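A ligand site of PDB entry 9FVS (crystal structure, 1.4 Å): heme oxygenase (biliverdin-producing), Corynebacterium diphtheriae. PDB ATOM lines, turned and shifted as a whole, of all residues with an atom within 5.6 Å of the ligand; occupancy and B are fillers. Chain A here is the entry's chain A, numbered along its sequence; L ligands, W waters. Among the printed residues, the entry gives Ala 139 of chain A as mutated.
The side-chain hydroxyl (OH) of Tyr 130 lies close to the backbone NH (N) of Lys 13 (3.4 Å).
O of Leu 134 sits at hydrogen-bond distance from OG of Ser 138.
OD1 of Asn 204 is in hydrogen-bond range of NH1 of Arg 132 (2.8 Å).
Residues that only touch the ligand: Gly 135 (3.2 Å), Val 131 (3.3 Å), Lys 13 (3.4 Å), Ala 23 (3.4 Å), Ile 143 (3.4 Å), Glu 24 (3.5 Å), Ala 139 (3.5 Å), Phe 208 (3.5 Å), Phe 201 (3.6 Å), Ser 138 (3.6 Å), Asn 204 (3.6 Å), Met 29 (3.6 Å), Val 142 (3.7 Å), Leu 33 (3.8 Å) and Leu 134 (3.8 Å).
Hydrophobic or aromatic side chains within 4 Å of the ligand: His 20, Ala 23, Met 29, Leu 33, Tyr 130, Val 131, Leu 134, Ala 139, Val 142, Ile 143, Phe 201 and Phe 208.
Of the 25 residues printed, 18 come within 4 Å of the ligand.
The nearest printed residue that does not touch the ligand is Arg 132 (4.2 Å).
Water W1 lies within hydrogen-bond range of O2 of the ligand and O of Ala 9.
Water W3 bridges the side-chain amino group (NZ) of Lys 13 (3.0 Å) and an oxygen (O1) of the ligand (3.5 Å).
A ring nitrogen (NE2) of His 20 is bound to a cobalt atom (CO1) of the ligand (2.3 Å).
O2 of the ligand lies within hydrogen-bond range of OH of Tyr 130 (2.7 Å).
O1 of the ligand is in salt-bridge range of NH1 of Arg 177 (3.1 Å).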
ATOM      1  N   ALA A   9     -13.127  20.388  27.006  1.00  0.00           N
ATOM      2  CA  ALA A   9     -11.917  20.541  26.202  1.00  0.00           C
ATOM      3  C   ALA A   9     -10.757  19.757  26.801  1.00  0.00           C
ATOM      4  O   ALA A   9      -9.989  19.102  26.076  1.00  0.00           O
ATOM      5  CB  ALA A   9     -11.553  22.012  26.031  1.00  0.00           C
ATOM      6  N   LEU A  12     -11.306  15.995  26.329  1.00  0.00           N
ATOM      7  CA  LEU A  12     -11.009  15.595  24.949  1.00  0.00           C
ATOM      8  C   LEU A  12      -9.508  15.458  24.726  1.00  0.00           C
ATOM      9  O   LEU A  12      -9.050  14.478  24.133  1.00  0.00           O
ATOM     10  CB  LEU A  12     -11.576  16.619  23.971  1.00  0.00           C
ATOM     11  CG  LEU A  12     -13.052  16.443  23.639  1.00  0.00           C
ATOM     12  CD1 LEU A  12     -13.613  17.727  23.037  1.00  0.00           C
ATOM     13  CD2 LEU A  12     -13.229  15.255  22.677  1.00  0.00           C
ATOM     14  N   LYS A  13      -8.731  16.438  25.182  1.00  0.00           N
ATOM     15  CA  LYS A  13      -7.287  16.398  24.974  1.00  0.00           C
ATOM     16  C   LYS A  13      -6.660  15.208  25.694  1.00  0.00           C
ATOM     17  O   LYS A  13      -5.814  14.509  25.134  1.00  0.00           O
ATOM     18  CB  LYS A  13      -6.656  17.702  25.457  1.00  0.00           C
ATOM     19  CG  LYS A  13      -5.192  17.822  25.088  1.00  0.00           C
ATOM     20  CD  LYS A  13      -4.571  19.122  25.556  1.00  0.00           C
ATOM     21  CE  LYS A  13      -3.104  19.205  25.166  1.00  0.00           C
ATOM     22  NZ  LYS A  13      -2.428  20.432  25.680  1.00  0.00           N
ATOM     23  N   HIS A  20      -3.316  10.611  19.434  1.00  0.00           N
ATOM     24  CA  HIS A  20      -2.531  11.649  18.787  1.00  0.00           C
ATOM     25  C   HIS A  20      -1.071  11.219  18.652  1.00  0.00           C
ATOM     26  O   HIS A  20      -0.464  11.382  17.582  1.00  0.00           O
ATOM     27  CB  HIS A  20      -2.643  12.951  19.576  1.00  0.00           C
ATOM     28  CG  HIS A  20      -1.987  14.101  18.889  1.00  0.00           C
ATOM     29  ND1 HIS A  20      -0.619  14.301  18.925  1.00  0.00           N
ATOM     30  CD2 HIS A  20      -2.491  15.075  18.104  1.00  0.00           C
ATOM     31  CE1 HIS A  20      -0.324  15.368  18.215  1.00  0.00           C
ATOM     32  NE2 HIS A  20      -1.442  15.856  17.711  1.00  0.00           N
ATOM     33  N   ALA A  23      -0.727   8.748  15.860  1.00  0.00           N
ATOM     34  CA  ALA A  23      -0.817   9.383  14.551  1.00  0.00           C
ATOM     35  C   ALA A  23       0.490  10.089  14.186  1.00  0.00           C
ATOM     36  O   ALA A  23       0.969   9.981  13.050  1.00  0.00           O
ATOM     37  CB  ALA A  23      -2.002  10.349  14.511  1.00  0.00           C
ATOM     38  N   GLU A  24       1.086  10.819  15.145  1.00  0.00           N
ATOM     39  CA  GLU A  24       2.357  11.482  14.866  1.00  0.00           C
ATOM     40  C   GLU A  24       3.446  10.470  14.518  1.00  0.00           C
ATOM     41  O   GLU A  24       4.320  10.754  13.684  1.00  0.00           O
ATOM     42  CB  GLU A  24       2.803  12.320  16.067  1.00  0.00           C
ATOM     43  CG  GLU A  24       2.296  13.744  16.052  1.00  0.00           C
ATOM     44  CD  GLU A  24       3.166  14.683  16.869  1.00  0.00           C
ATOM     45  OE1 GLU A  24       4.336  14.904  16.492  1.00  0.00           O
ATOM     46  OE2 GLU A  24       2.680  15.191  17.895  1.00  0.00           O
ATOM     47  N   MET A  29       3.380   9.579   7.991  1.00  0.00           N
ATOM     48  CA  MET A  29       3.453  10.970   8.422  1.00  0.00           C
ATOM     49  C   MET A  29       4.840  11.321   8.944  1.00  0.00           C
ATOM     50  O   MET A  29       5.364  12.406   8.667  1.00  0.00           O
ATOM     51  CB  MET A  29       2.359  11.288   9.443  1.00  0.00           C
ATOM     52  CG  MET A  29       1.997  12.763   9.551  1.00  0.00           C
ATOM     53  SD  MET A  29       1.676  13.630   7.999  1.00  0.00           S
ATOM     54  CE  MET A  29       0.684  12.462   7.087  1.00  0.00           C
ATOM     55  N   LEU A  33       7.014  14.237   7.172  1.00  0.00           N
ATOM     56  CA  LEU A  33       7.401  15.445   7.890  1.00  0.00           C
ATOM     57  C   LEU A  33       8.912  15.552   8.050  1.00  0.00           C
ATOM     58  O   LEU A  33       9.447  16.664   8.124  1.00  0.00           O
ATOM     59  CB  LEU A  33       6.728  15.478   9.257  1.00  0.00           C
ATOM     60  CG  LEU A  33       5.209  15.670   9.214  1.00  0.00           C
ATOM     61  CD1 LEU A  33       4.661  15.819  10.623  1.00  0.00           C
ATOM     62  CD2 LEU A  33       4.827  16.867   8.351  1.00  0.00           C
ATOM     63  N   TYR A 130     -13.609  19.073  16.364  1.00  0.00           N
ATOM     64  CA  TYR A 130     -12.465  19.218  17.250  1.00  0.00           C
ATOM     65  C   TYR A 130     -11.239  18.511  16.680  1.00  0.00           C
ATOM     66  O   TYR A 130     -10.156  19.094  16.580  1.00  0.00           O
ATOM     67  CB  TYR A 130     -12.825  18.665  18.627  1.00  0.00           C
ATOM     68  CG  TYR A 130     -11.635  18.343  19.506  1.00  0.00           C
ATOM     69  CD1 TYR A 130     -11.001  19.335  20.251  1.00  0.00           C
ATOM     70  CD2 TYR A 130     -11.167  17.039  19.611  1.00  0.00           C
ATOM     71  CE1 TYR A 130      -9.902  19.028  21.059  1.00  0.00           C
ATOM     72  CE2 TYR A 130     -10.082  16.723  20.424  1.00  0.00           C
ATOM     73  CZ  TYR A 130      -9.455  17.714  21.146  1.00  0.00           C
ATOM     74  OH  TYR A 130      -8.378  17.398  21.936  1.00  0.00           O
ATOM     75  N   VAL A 131     -11.411  17.236  16.303  1.00  0.00           N
ATOM     76  CA  VAL A 131     -10.262  16.425  15.899  1.00  0.00           C
ATOM     77  C   VAL A 131      -9.561  17.030  14.680  1.00  0.00           C
ATOM     78  O   VAL A 131      -8.331  17.088  14.632  1.00  0.00           O
ATOM     79  CB  VAL A 131     -10.697  14.956  15.680  1.00  0.00           C
ATOM     80  CG1 VAL A 131      -9.587  14.143  15.032  1.00  0.00           C
ATOM     81  CG2 VAL A 131     -11.078  14.320  17.029  1.00  0.00           C
ATOM     82  N   ARG A 132     -10.333  17.529  13.705  1.00  0.00           N
ATOM     83  CA  ARG A 132      -9.697  18.108  12.517  1.00  0.00           C
ATOM     84  C   ARG A 132      -9.260  19.553  12.739  1.00  0.00           C
ATOM     85  O   ARG A 132      -8.083  19.876  12.596  1.00  0.00           O
ATOM     86  CB  ARG A 132     -10.590  17.991  11.271  1.00  0.00           C
ATOM     87  CG  ARG A 132     -10.671  16.592  10.654  1.00  0.00           C
ATOM     88  CD  ARG A 132      -9.307  15.911  10.435  1.00  0.00           C
ATOM     89  NE  ARG A 132      -8.310  16.826   9.887  1.00  0.00           N
ATOM     90  CZ  ARG A 132      -7.037  16.518   9.701  1.00  0.00           C
ATOM     91  NH1 ARG A 132      -6.581  15.296   9.923  1.00  0.00           N
ATOM     92  NH2 ARG A 132      -6.189  17.458   9.286  1.00  0.00           N
ATOM     93  N   LEU A 134      -9.172  21.812  15.379  1.00  0.00           N
ATOM     94  CA  LEU A 134      -8.265  22.264  16.437  1.00  0.00           C
ATOM     95  C   LEU A 134      -6.855  21.749  16.179  1.00  0.00           C
ATOM     96  O   LEU A 134      -5.872  22.455  16.454  1.00  0.00           O
ATOM     97  CB  LEU A 134      -8.778  21.907  17.835  1.00  0.00           C
ATOM     98  CG  LEU A 134      -7.998  22.623  18.951  1.00  0.00           C
ATOM     99  CD1 LEU A 134      -8.065  24.124  18.762  1.00  0.00           C
ATOM    100  CD2 LEU A 134      -8.485  22.241  20.338  1.00  0.00           C
ATOM    101  N   GLY A 135      -6.745  20.545  15.611  1.00  0.00           N
ATOM    102  CA  GLY A 135      -5.450  20.076  15.148  1.00  0.00           C
ATOM    103  C   GLY A 135      -4.863  20.950  14.056  1.00  0.00           C
ATOM    104  O   GLY A 135      -3.675  21.285  14.089  1.00  0.00           O
ATOM    105  N   ASP A 136      -5.689  21.343  13.080  1.00  0.00           N
ATOM    106  CA  ASP A 136      -5.212  22.215  12.014  1.00  0.00           C
ATOM    107  C   ASP A 136      -4.694  23.533  12.571  1.00  0.00           C
ATOM    108  O   ASP A 136      -3.615  24.001  12.180  1.00  0.00           O
ATOM    109  CB  ASP A 136      -6.329  22.516  11.019  1.00  0.00           C
ATOM    110  CG  ASP A 136      -6.809  21.294  10.253  1.00  0.00           C
ATOM    111  OD1 ASP A 136      -6.048  20.313  10.125  1.00  0.00           O
ATOM    112  OD2 ASP A 136      -7.958  21.342   9.753  1.00  0.00           O
ATOM    113  N   SER A 138      -3.504  24.037  15.450  1.00  0.00           N
ATOM    114  CA  SER A 138      -2.355  23.777  16.305  1.00  0.00           C
ATOM    115  C   SER A 138      -1.094  23.461  15.526  1.00  0.00           C
ATOM    116  O   SER A 138       0.006  23.805  15.969  1.00  0.00           O
ATOM    117  CB  SER A 138      -2.673  22.605  17.235  1.00  0.00           C
ATOM    118  OG  SER A 138      -3.729  22.911  18.112  1.00  0.00           O
ATOM    119  N   ALA A 139      -1.217  22.771  14.380  1.00  0.00           N
ATOM    120  CA  ALA A 139      -0.083  22.192  13.698  1.00  0.00           C
ATOM    121  C   ALA A 139       0.260  22.859  12.382  1.00  0.00           C
ATOM    122  O   ALA A 139       1.291  22.536  11.793  1.00  0.00           O
ATOM    123  CB  ALA A 139      -0.349  20.697  13.427  1.00  0.00           C
ATOM    124  N   VAL A 142       3.787  24.632  11.746  1.00  0.00           N
ATOM    125  CA  VAL A 142       4.948  23.747  11.761  1.00  0.00           C
ATOM    126  C   VAL A 142       4.936  22.808  10.558  1.00  0.00           C
ATOM    127  O   VAL A 142       5.977  22.598   9.919  1.00  0.00           O
ATOM    128  CB  VAL A 142       5.109  23.023  13.115  1.00  0.00           C
ATOM    129  CG1 VAL A 142       5.327  24.038  14.229  1.00  0.00           C
ATOM    130  CG2 VAL A 142       3.915  22.138  13.412  1.00  0.00           C
ATOM    131  N   ILE A 143       3.781  22.261  10.204  1.00  0.00           N
ATOM    132  CA  ILE A 143       3.744  21.339   9.064  1.00  0.00           C
ATOM    133  C   ILE A 143       4.033  22.073   7.754  1.00  0.00           C
ATOM    134  O   ILE A 143       4.818  21.593   6.923  1.00  0.00           O
ATOM    135  CB  ILE A 143       2.412  20.566   9.019  1.00  0.00           C
ATOM    136  CG1 ILE A 143       2.291  19.656  10.242  1.00  0.00           C
ATOM    137  CG2 ILE A 143       2.344  19.728   7.757  1.00  0.00           C
ATOM    138  CD1 ILE A 143       0.955  18.952  10.376  1.00  0.00           C
ATOM    139  N   MET A 146       7.693  22.654   7.370  1.00  0.00           N
ATOM    140  CA  MET A 146       8.367  21.394   6.949  1.00  0.00           C
ATOM    141  C   MET A 146       8.253  21.032   5.419  1.00  0.00           C
ATOM    142  O   MET A 146       9.194  20.609   4.652  1.00  0.00           O
ATOM    143  CB  MET A 146       7.890  20.216   7.798  1.00  0.00           C
ATOM    144  CG  MET A 146       8.425  20.313   9.210  1.00  0.00           C
ATOM    145  SD  MET A 146       8.164  18.868  10.256  1.00  0.00           S
ATOM    146  CE  MET A 146       7.388  19.678  11.665  1.00  0.00           C
ATOM    147  N   LYS A 173      -7.651  29.603  19.540  1.00  0.00           N
ATOM    148  CA  LYS A 173      -7.678  28.226  20.063  1.00  0.00           C
ATOM    149  C   LYS A 173      -8.208  28.202  21.490  1.00  0.00           C
ATOM    150  O   LYS A 173      -9.008  27.324  21.849  1.00  0.00           O
ATOM    151  CB  LYS A 173      -6.274  27.618  20.013  1.00  0.00           C
ATOM    152  CG  LYS A 173      -5.709  27.360  18.619  1.00  0.00           C
ATOM    153  CD  LYS A 173      -4.357  26.611  18.696  1.00  0.00           C
ATOM    154  CE  LYS A 173      -3.287  27.412  19.446  1.00  0.00           C
ATOM    155  NZ  LYS A 173      -1.995  26.648  19.548  1.00  0.00           N
ATOM    156  N   ARG A 177     -11.548  26.231  22.677  1.00  0.00           N
ATOM    157  CA  ARG A 177     -11.630  25.293  23.795  1.00  0.00           C
ATOM    158  C   ARG A 177     -12.706  25.725  24.789  1.00  0.00           C
ATOM    159  O   ARG A 177     -13.434  24.886  25.325  1.00  0.00           O
ATOM    160  CB  ARG A 177     -10.249  25.102  24.436  1.00  0.00           C
ATOM    161  CG  ARG A 177      -9.301  24.271  23.552  1.00  0.00           C
ATOM    162  CD  ARG A 177      -7.941  24.018  24.203  1.00  0.00           C
ATOM    163  NE  ARG A 177      -7.019  25.144  24.041  1.00  0.00           N
ATOM    164  CZ  ARG A 177      -5.998  25.178  23.190  1.00  0.00           C
ATOM    165  NH1 ARG A 177      -5.720  24.145  22.411  1.00  0.00           N
ATOM    166  NH2 ARG A 177      -5.249  26.271  23.127  1.00  0.00           N
ATOM    167  N   PHE A 201     -10.056  10.007  15.473  1.00  0.00           N
ATOM    168  CA  PHE A 201      -8.614   9.808  15.379  1.00  0.00           C
ATOM    169  C   PHE A 201      -8.278   8.512  14.655  1.00  0.00           C
ATOM    170  O   PHE A 201      -7.329   8.478  13.864  1.00  0.00           O
ATOM    171  CB  PHE A 201      -7.988   9.820  16.778  1.00  0.00           C
ATOM    172  CG  PHE A 201      -7.441  11.160  17.188  1.00  0.00           C
ATOM    173  CD1 PHE A 201      -6.179  11.559  16.766  1.00  0.00           C
ATOM    174  CD2 PHE A 201      -8.195  12.022  17.965  1.00  0.00           C
ATOM    175  CE1 PHE A 201      -5.665  12.804  17.130  1.00  0.00           C
ATOM    176  CE2 PHE A 201      -7.691  13.269  18.328  1.00  0.00           C
ATOM    177  CZ  PHE A 201      -6.421  13.662  17.917  1.00  0.00           C
ATOM    178  N   ASN A 204      -8.586   9.005  10.959  1.00  0.00           N
ATOM    179  CA  ASN A 204      -7.466   9.776  10.420  1.00  0.00           C
ATOM    180  C   ASN A 204      -6.184   8.953  10.386  1.00  0.00           C
ATOM    181  O   ASN A 204      -5.418   9.030   9.413  1.00  0.00           O
ATOM    182  CB  ASN A 204      -7.286  11.067  11.210  1.00  0.00           C
ATOM    183  CG  ASN A 204      -8.230  12.137  10.755  1.00  0.00           C
ATOM    184  OD1 ASN A 204      -7.954  12.858   9.802  1.00  0.00           O
ATOM    185  ND2 ASN A 204      -9.382  12.239  11.412  1.00  0.00           N
ATOM    186  N   HIS A 205      -5.935   8.162  11.431  1.00  0.00           N
ATOM    187  CA  HIS A 205      -4.756   7.292  11.422  1.00  0.00           C
ATOM    188  C   HIS A 205      -4.780   6.353  10.227  1.00  0.00           C
ATOM    189  O   HIS A 205      -3.753   6.121   9.568  1.00  0.00           O
ATOM    190  CB  HIS A 205      -4.705   6.500  12.741  1.00  0.00           C
ATOM    191  CG  HIS A 205      -3.391   5.810  12.987  1.00  0.00           C
ATOM    192  ND1 HIS A 205      -2.932   5.561  14.260  1.00  0.00           N
ATOM    193  CD2 HIS A 205      -2.467   5.297  12.148  1.00  0.00           C
ATOM    194  CE1 HIS A 205      -1.765   4.933  14.191  1.00  0.00           C
ATOM    195  NE2 HIS A 205      -1.465   4.766  12.922  1.00  0.00           N
ATOM    196  N   PHE A 208      -3.555   7.822   6.937  1.00  0.00           N
ATOM    197  CA  PHE A 208      -2.095   7.755   6.854  1.00  0.00           C
ATOM    198  C   PHE A 208      -1.635   6.335   6.550  1.00  0.00           C
ATOM    199  O   PHE A 208      -0.695   6.145   5.775  1.00  0.00           O
ATOM    200  CB  PHE A 208      -1.459   8.199   8.167  1.00  0.00           C
ATOM    201  CG  PHE A 208      -1.731   9.610   8.544  1.00  0.00           C
ATOM    202  CD1 PHE A 208      -2.158  10.528   7.611  1.00  0.00           C
ATOM    203  CD2 PHE A 208      -1.548  10.029   9.861  1.00  0.00           C
ATOM    204  CE1 PHE A 208      -2.418  11.840   7.984  1.00  0.00           C
ATOM    205  CE2 PHE A 208      -1.780  11.325  10.225  1.00  0.00           C
ATOM    206  CZ  PHE A 208      -2.218  12.236   9.288  1.00  0.00           C
HETATM  207 CO1  LIG L   1      -1.985  17.386  16.117  1.00  0.00          CO
HETATM  208  C1  LIG L   1      -2.562  19.396  18.806  1.00  0.00           C
HETATM  209  C2  LIG L   1      -5.298  16.606  15.938  1.00  0.00           C
HETATM  210  C3  LIG L   1      -1.258  14.981  13.819  1.00  0.00           C
HETATM  211  C4  LIG L   1       1.190  18.662  15.822  1.00  0.00           C
HETATM  212  N1  LIG L   1      -3.561  17.886  17.132  1.00  0.00           N
HETATM  213  C5  LIG L   1      -3.688  18.723  18.199  1.00  0.00           C
HETATM  214  C6  LIG L   1      -5.036  18.903  18.778  1.00  0.00           C
HETATM  215  C7  LIG L   1      -5.842  18.051  17.916  1.00  0.00           C
HETATM  216  C8  LIG L   1      -4.845  17.496  16.985  1.00  0.00           C
HETATM  217  C9  LIG L   1      -7.314  17.793  17.967  1.00  0.00           C
HETATM  218  C10 LIG L   1      -5.485  19.763  19.926  1.00  0.00           C
HETATM  219  C11 LIG L   1      -5.351  19.080  21.275  1.00  0.00           C
HETATM  220  C12 LIG L   1      -6.043  19.997  22.254  1.00  0.00           C
HETATM  221  O1  LIG L   1      -5.500  21.098  22.540  1.00  0.00           O
HETATM  222  O2  LIG L   1      -7.128  19.619  22.733  1.00  0.00           O
HETATM  223  N2  LIG L   1      -3.037  16.114  15.108  1.00  0.00           N
HETATM  224  C13 LIG L   1      -4.382  15.864  15.105  1.00  0.00           C
HETATM  225  C14 LIG L   1      -4.908  14.810  14.207  1.00  0.00           C
HETATM  226  C15 LIG L   1      -3.676  14.343  13.602  1.00  0.00           C
HETATM  227  C16 LIG L   1      -2.639  15.178  14.215  1.00  0.00           C
HETATM  228  C17 LIG L   1      -6.319  14.348  13.988  1.00  0.00           C
HETATM  229  C18 LIG L   1      -3.512  13.278  12.595  1.00  0.00           C
HETATM  230  C19 LIG L   1      -4.221  12.163  12.693  1.00  0.00           C
HETATM  231  N3  LIG L   1      -0.424  16.929  15.080  1.00  0.00           N
HETATM  232  C20 LIG L   1      -0.235  15.923  14.171  1.00  0.00           C
HETATM  233  C21 LIG L   1       1.079  15.794  13.502  1.00  0.00           C
HETATM  234  C22 LIG L   1       1.781  16.906  14.106  1.00  0.00           C
HETATM  235  C23 LIG L   1       0.816  17.497  15.033  1.00  0.00           C
HETATM  236  C24 LIG L   1       1.523  14.779  12.490  1.00  0.00           C
HETATM  237  C25 LIG L   1       3.188  17.324  13.895  1.00  0.00           C
HETATM  238  C26 LIG L   1       3.458  18.441  13.247  1.00  0.00           C
HETATM  239  N4  LIG L   1      -0.934  18.704  17.087  1.00  0.00           N
HETATM  240  C27 LIG L   1       0.332  19.146  16.882  1.00  0.00           C
HETATM  241  C28 LIG L   1       0.867  20.177  17.807  1.00  0.00           C
HETATM  242  C29 LIG L   1      -0.262  20.395  18.706  1.00  0.00           C
HETATM  243  C30 LIG L   1      -1.265  19.462  18.158  1.00  0.00           C
HETATM  244  C31 LIG L   1       2.221  20.834  17.824  1.00  0.00           C
HETATM  245  C32 LIG L   1      -0.401  21.314  19.889  1.00  0.00           C
HETATM  246  C33 LIG L   1       0.197  20.648  21.127  1.00  0.00           C
HETATM  247  C34 LIG L   1      -0.458  19.313  21.408  1.00  0.00           C
HETATM  248  O3  LIG L   1      -1.564  19.294  21.998  1.00  0.00           O
HETATM  249  O   HOH W   1      -8.390  20.849  24.609  1.00  0.00           O
HETATM  250  O   HOH W   2      -2.818  21.417  22.288  1.00  0.00           O
HETATM  251  O   HOH W   3      -4.435  22.626  25.483  1.00  0.00           O
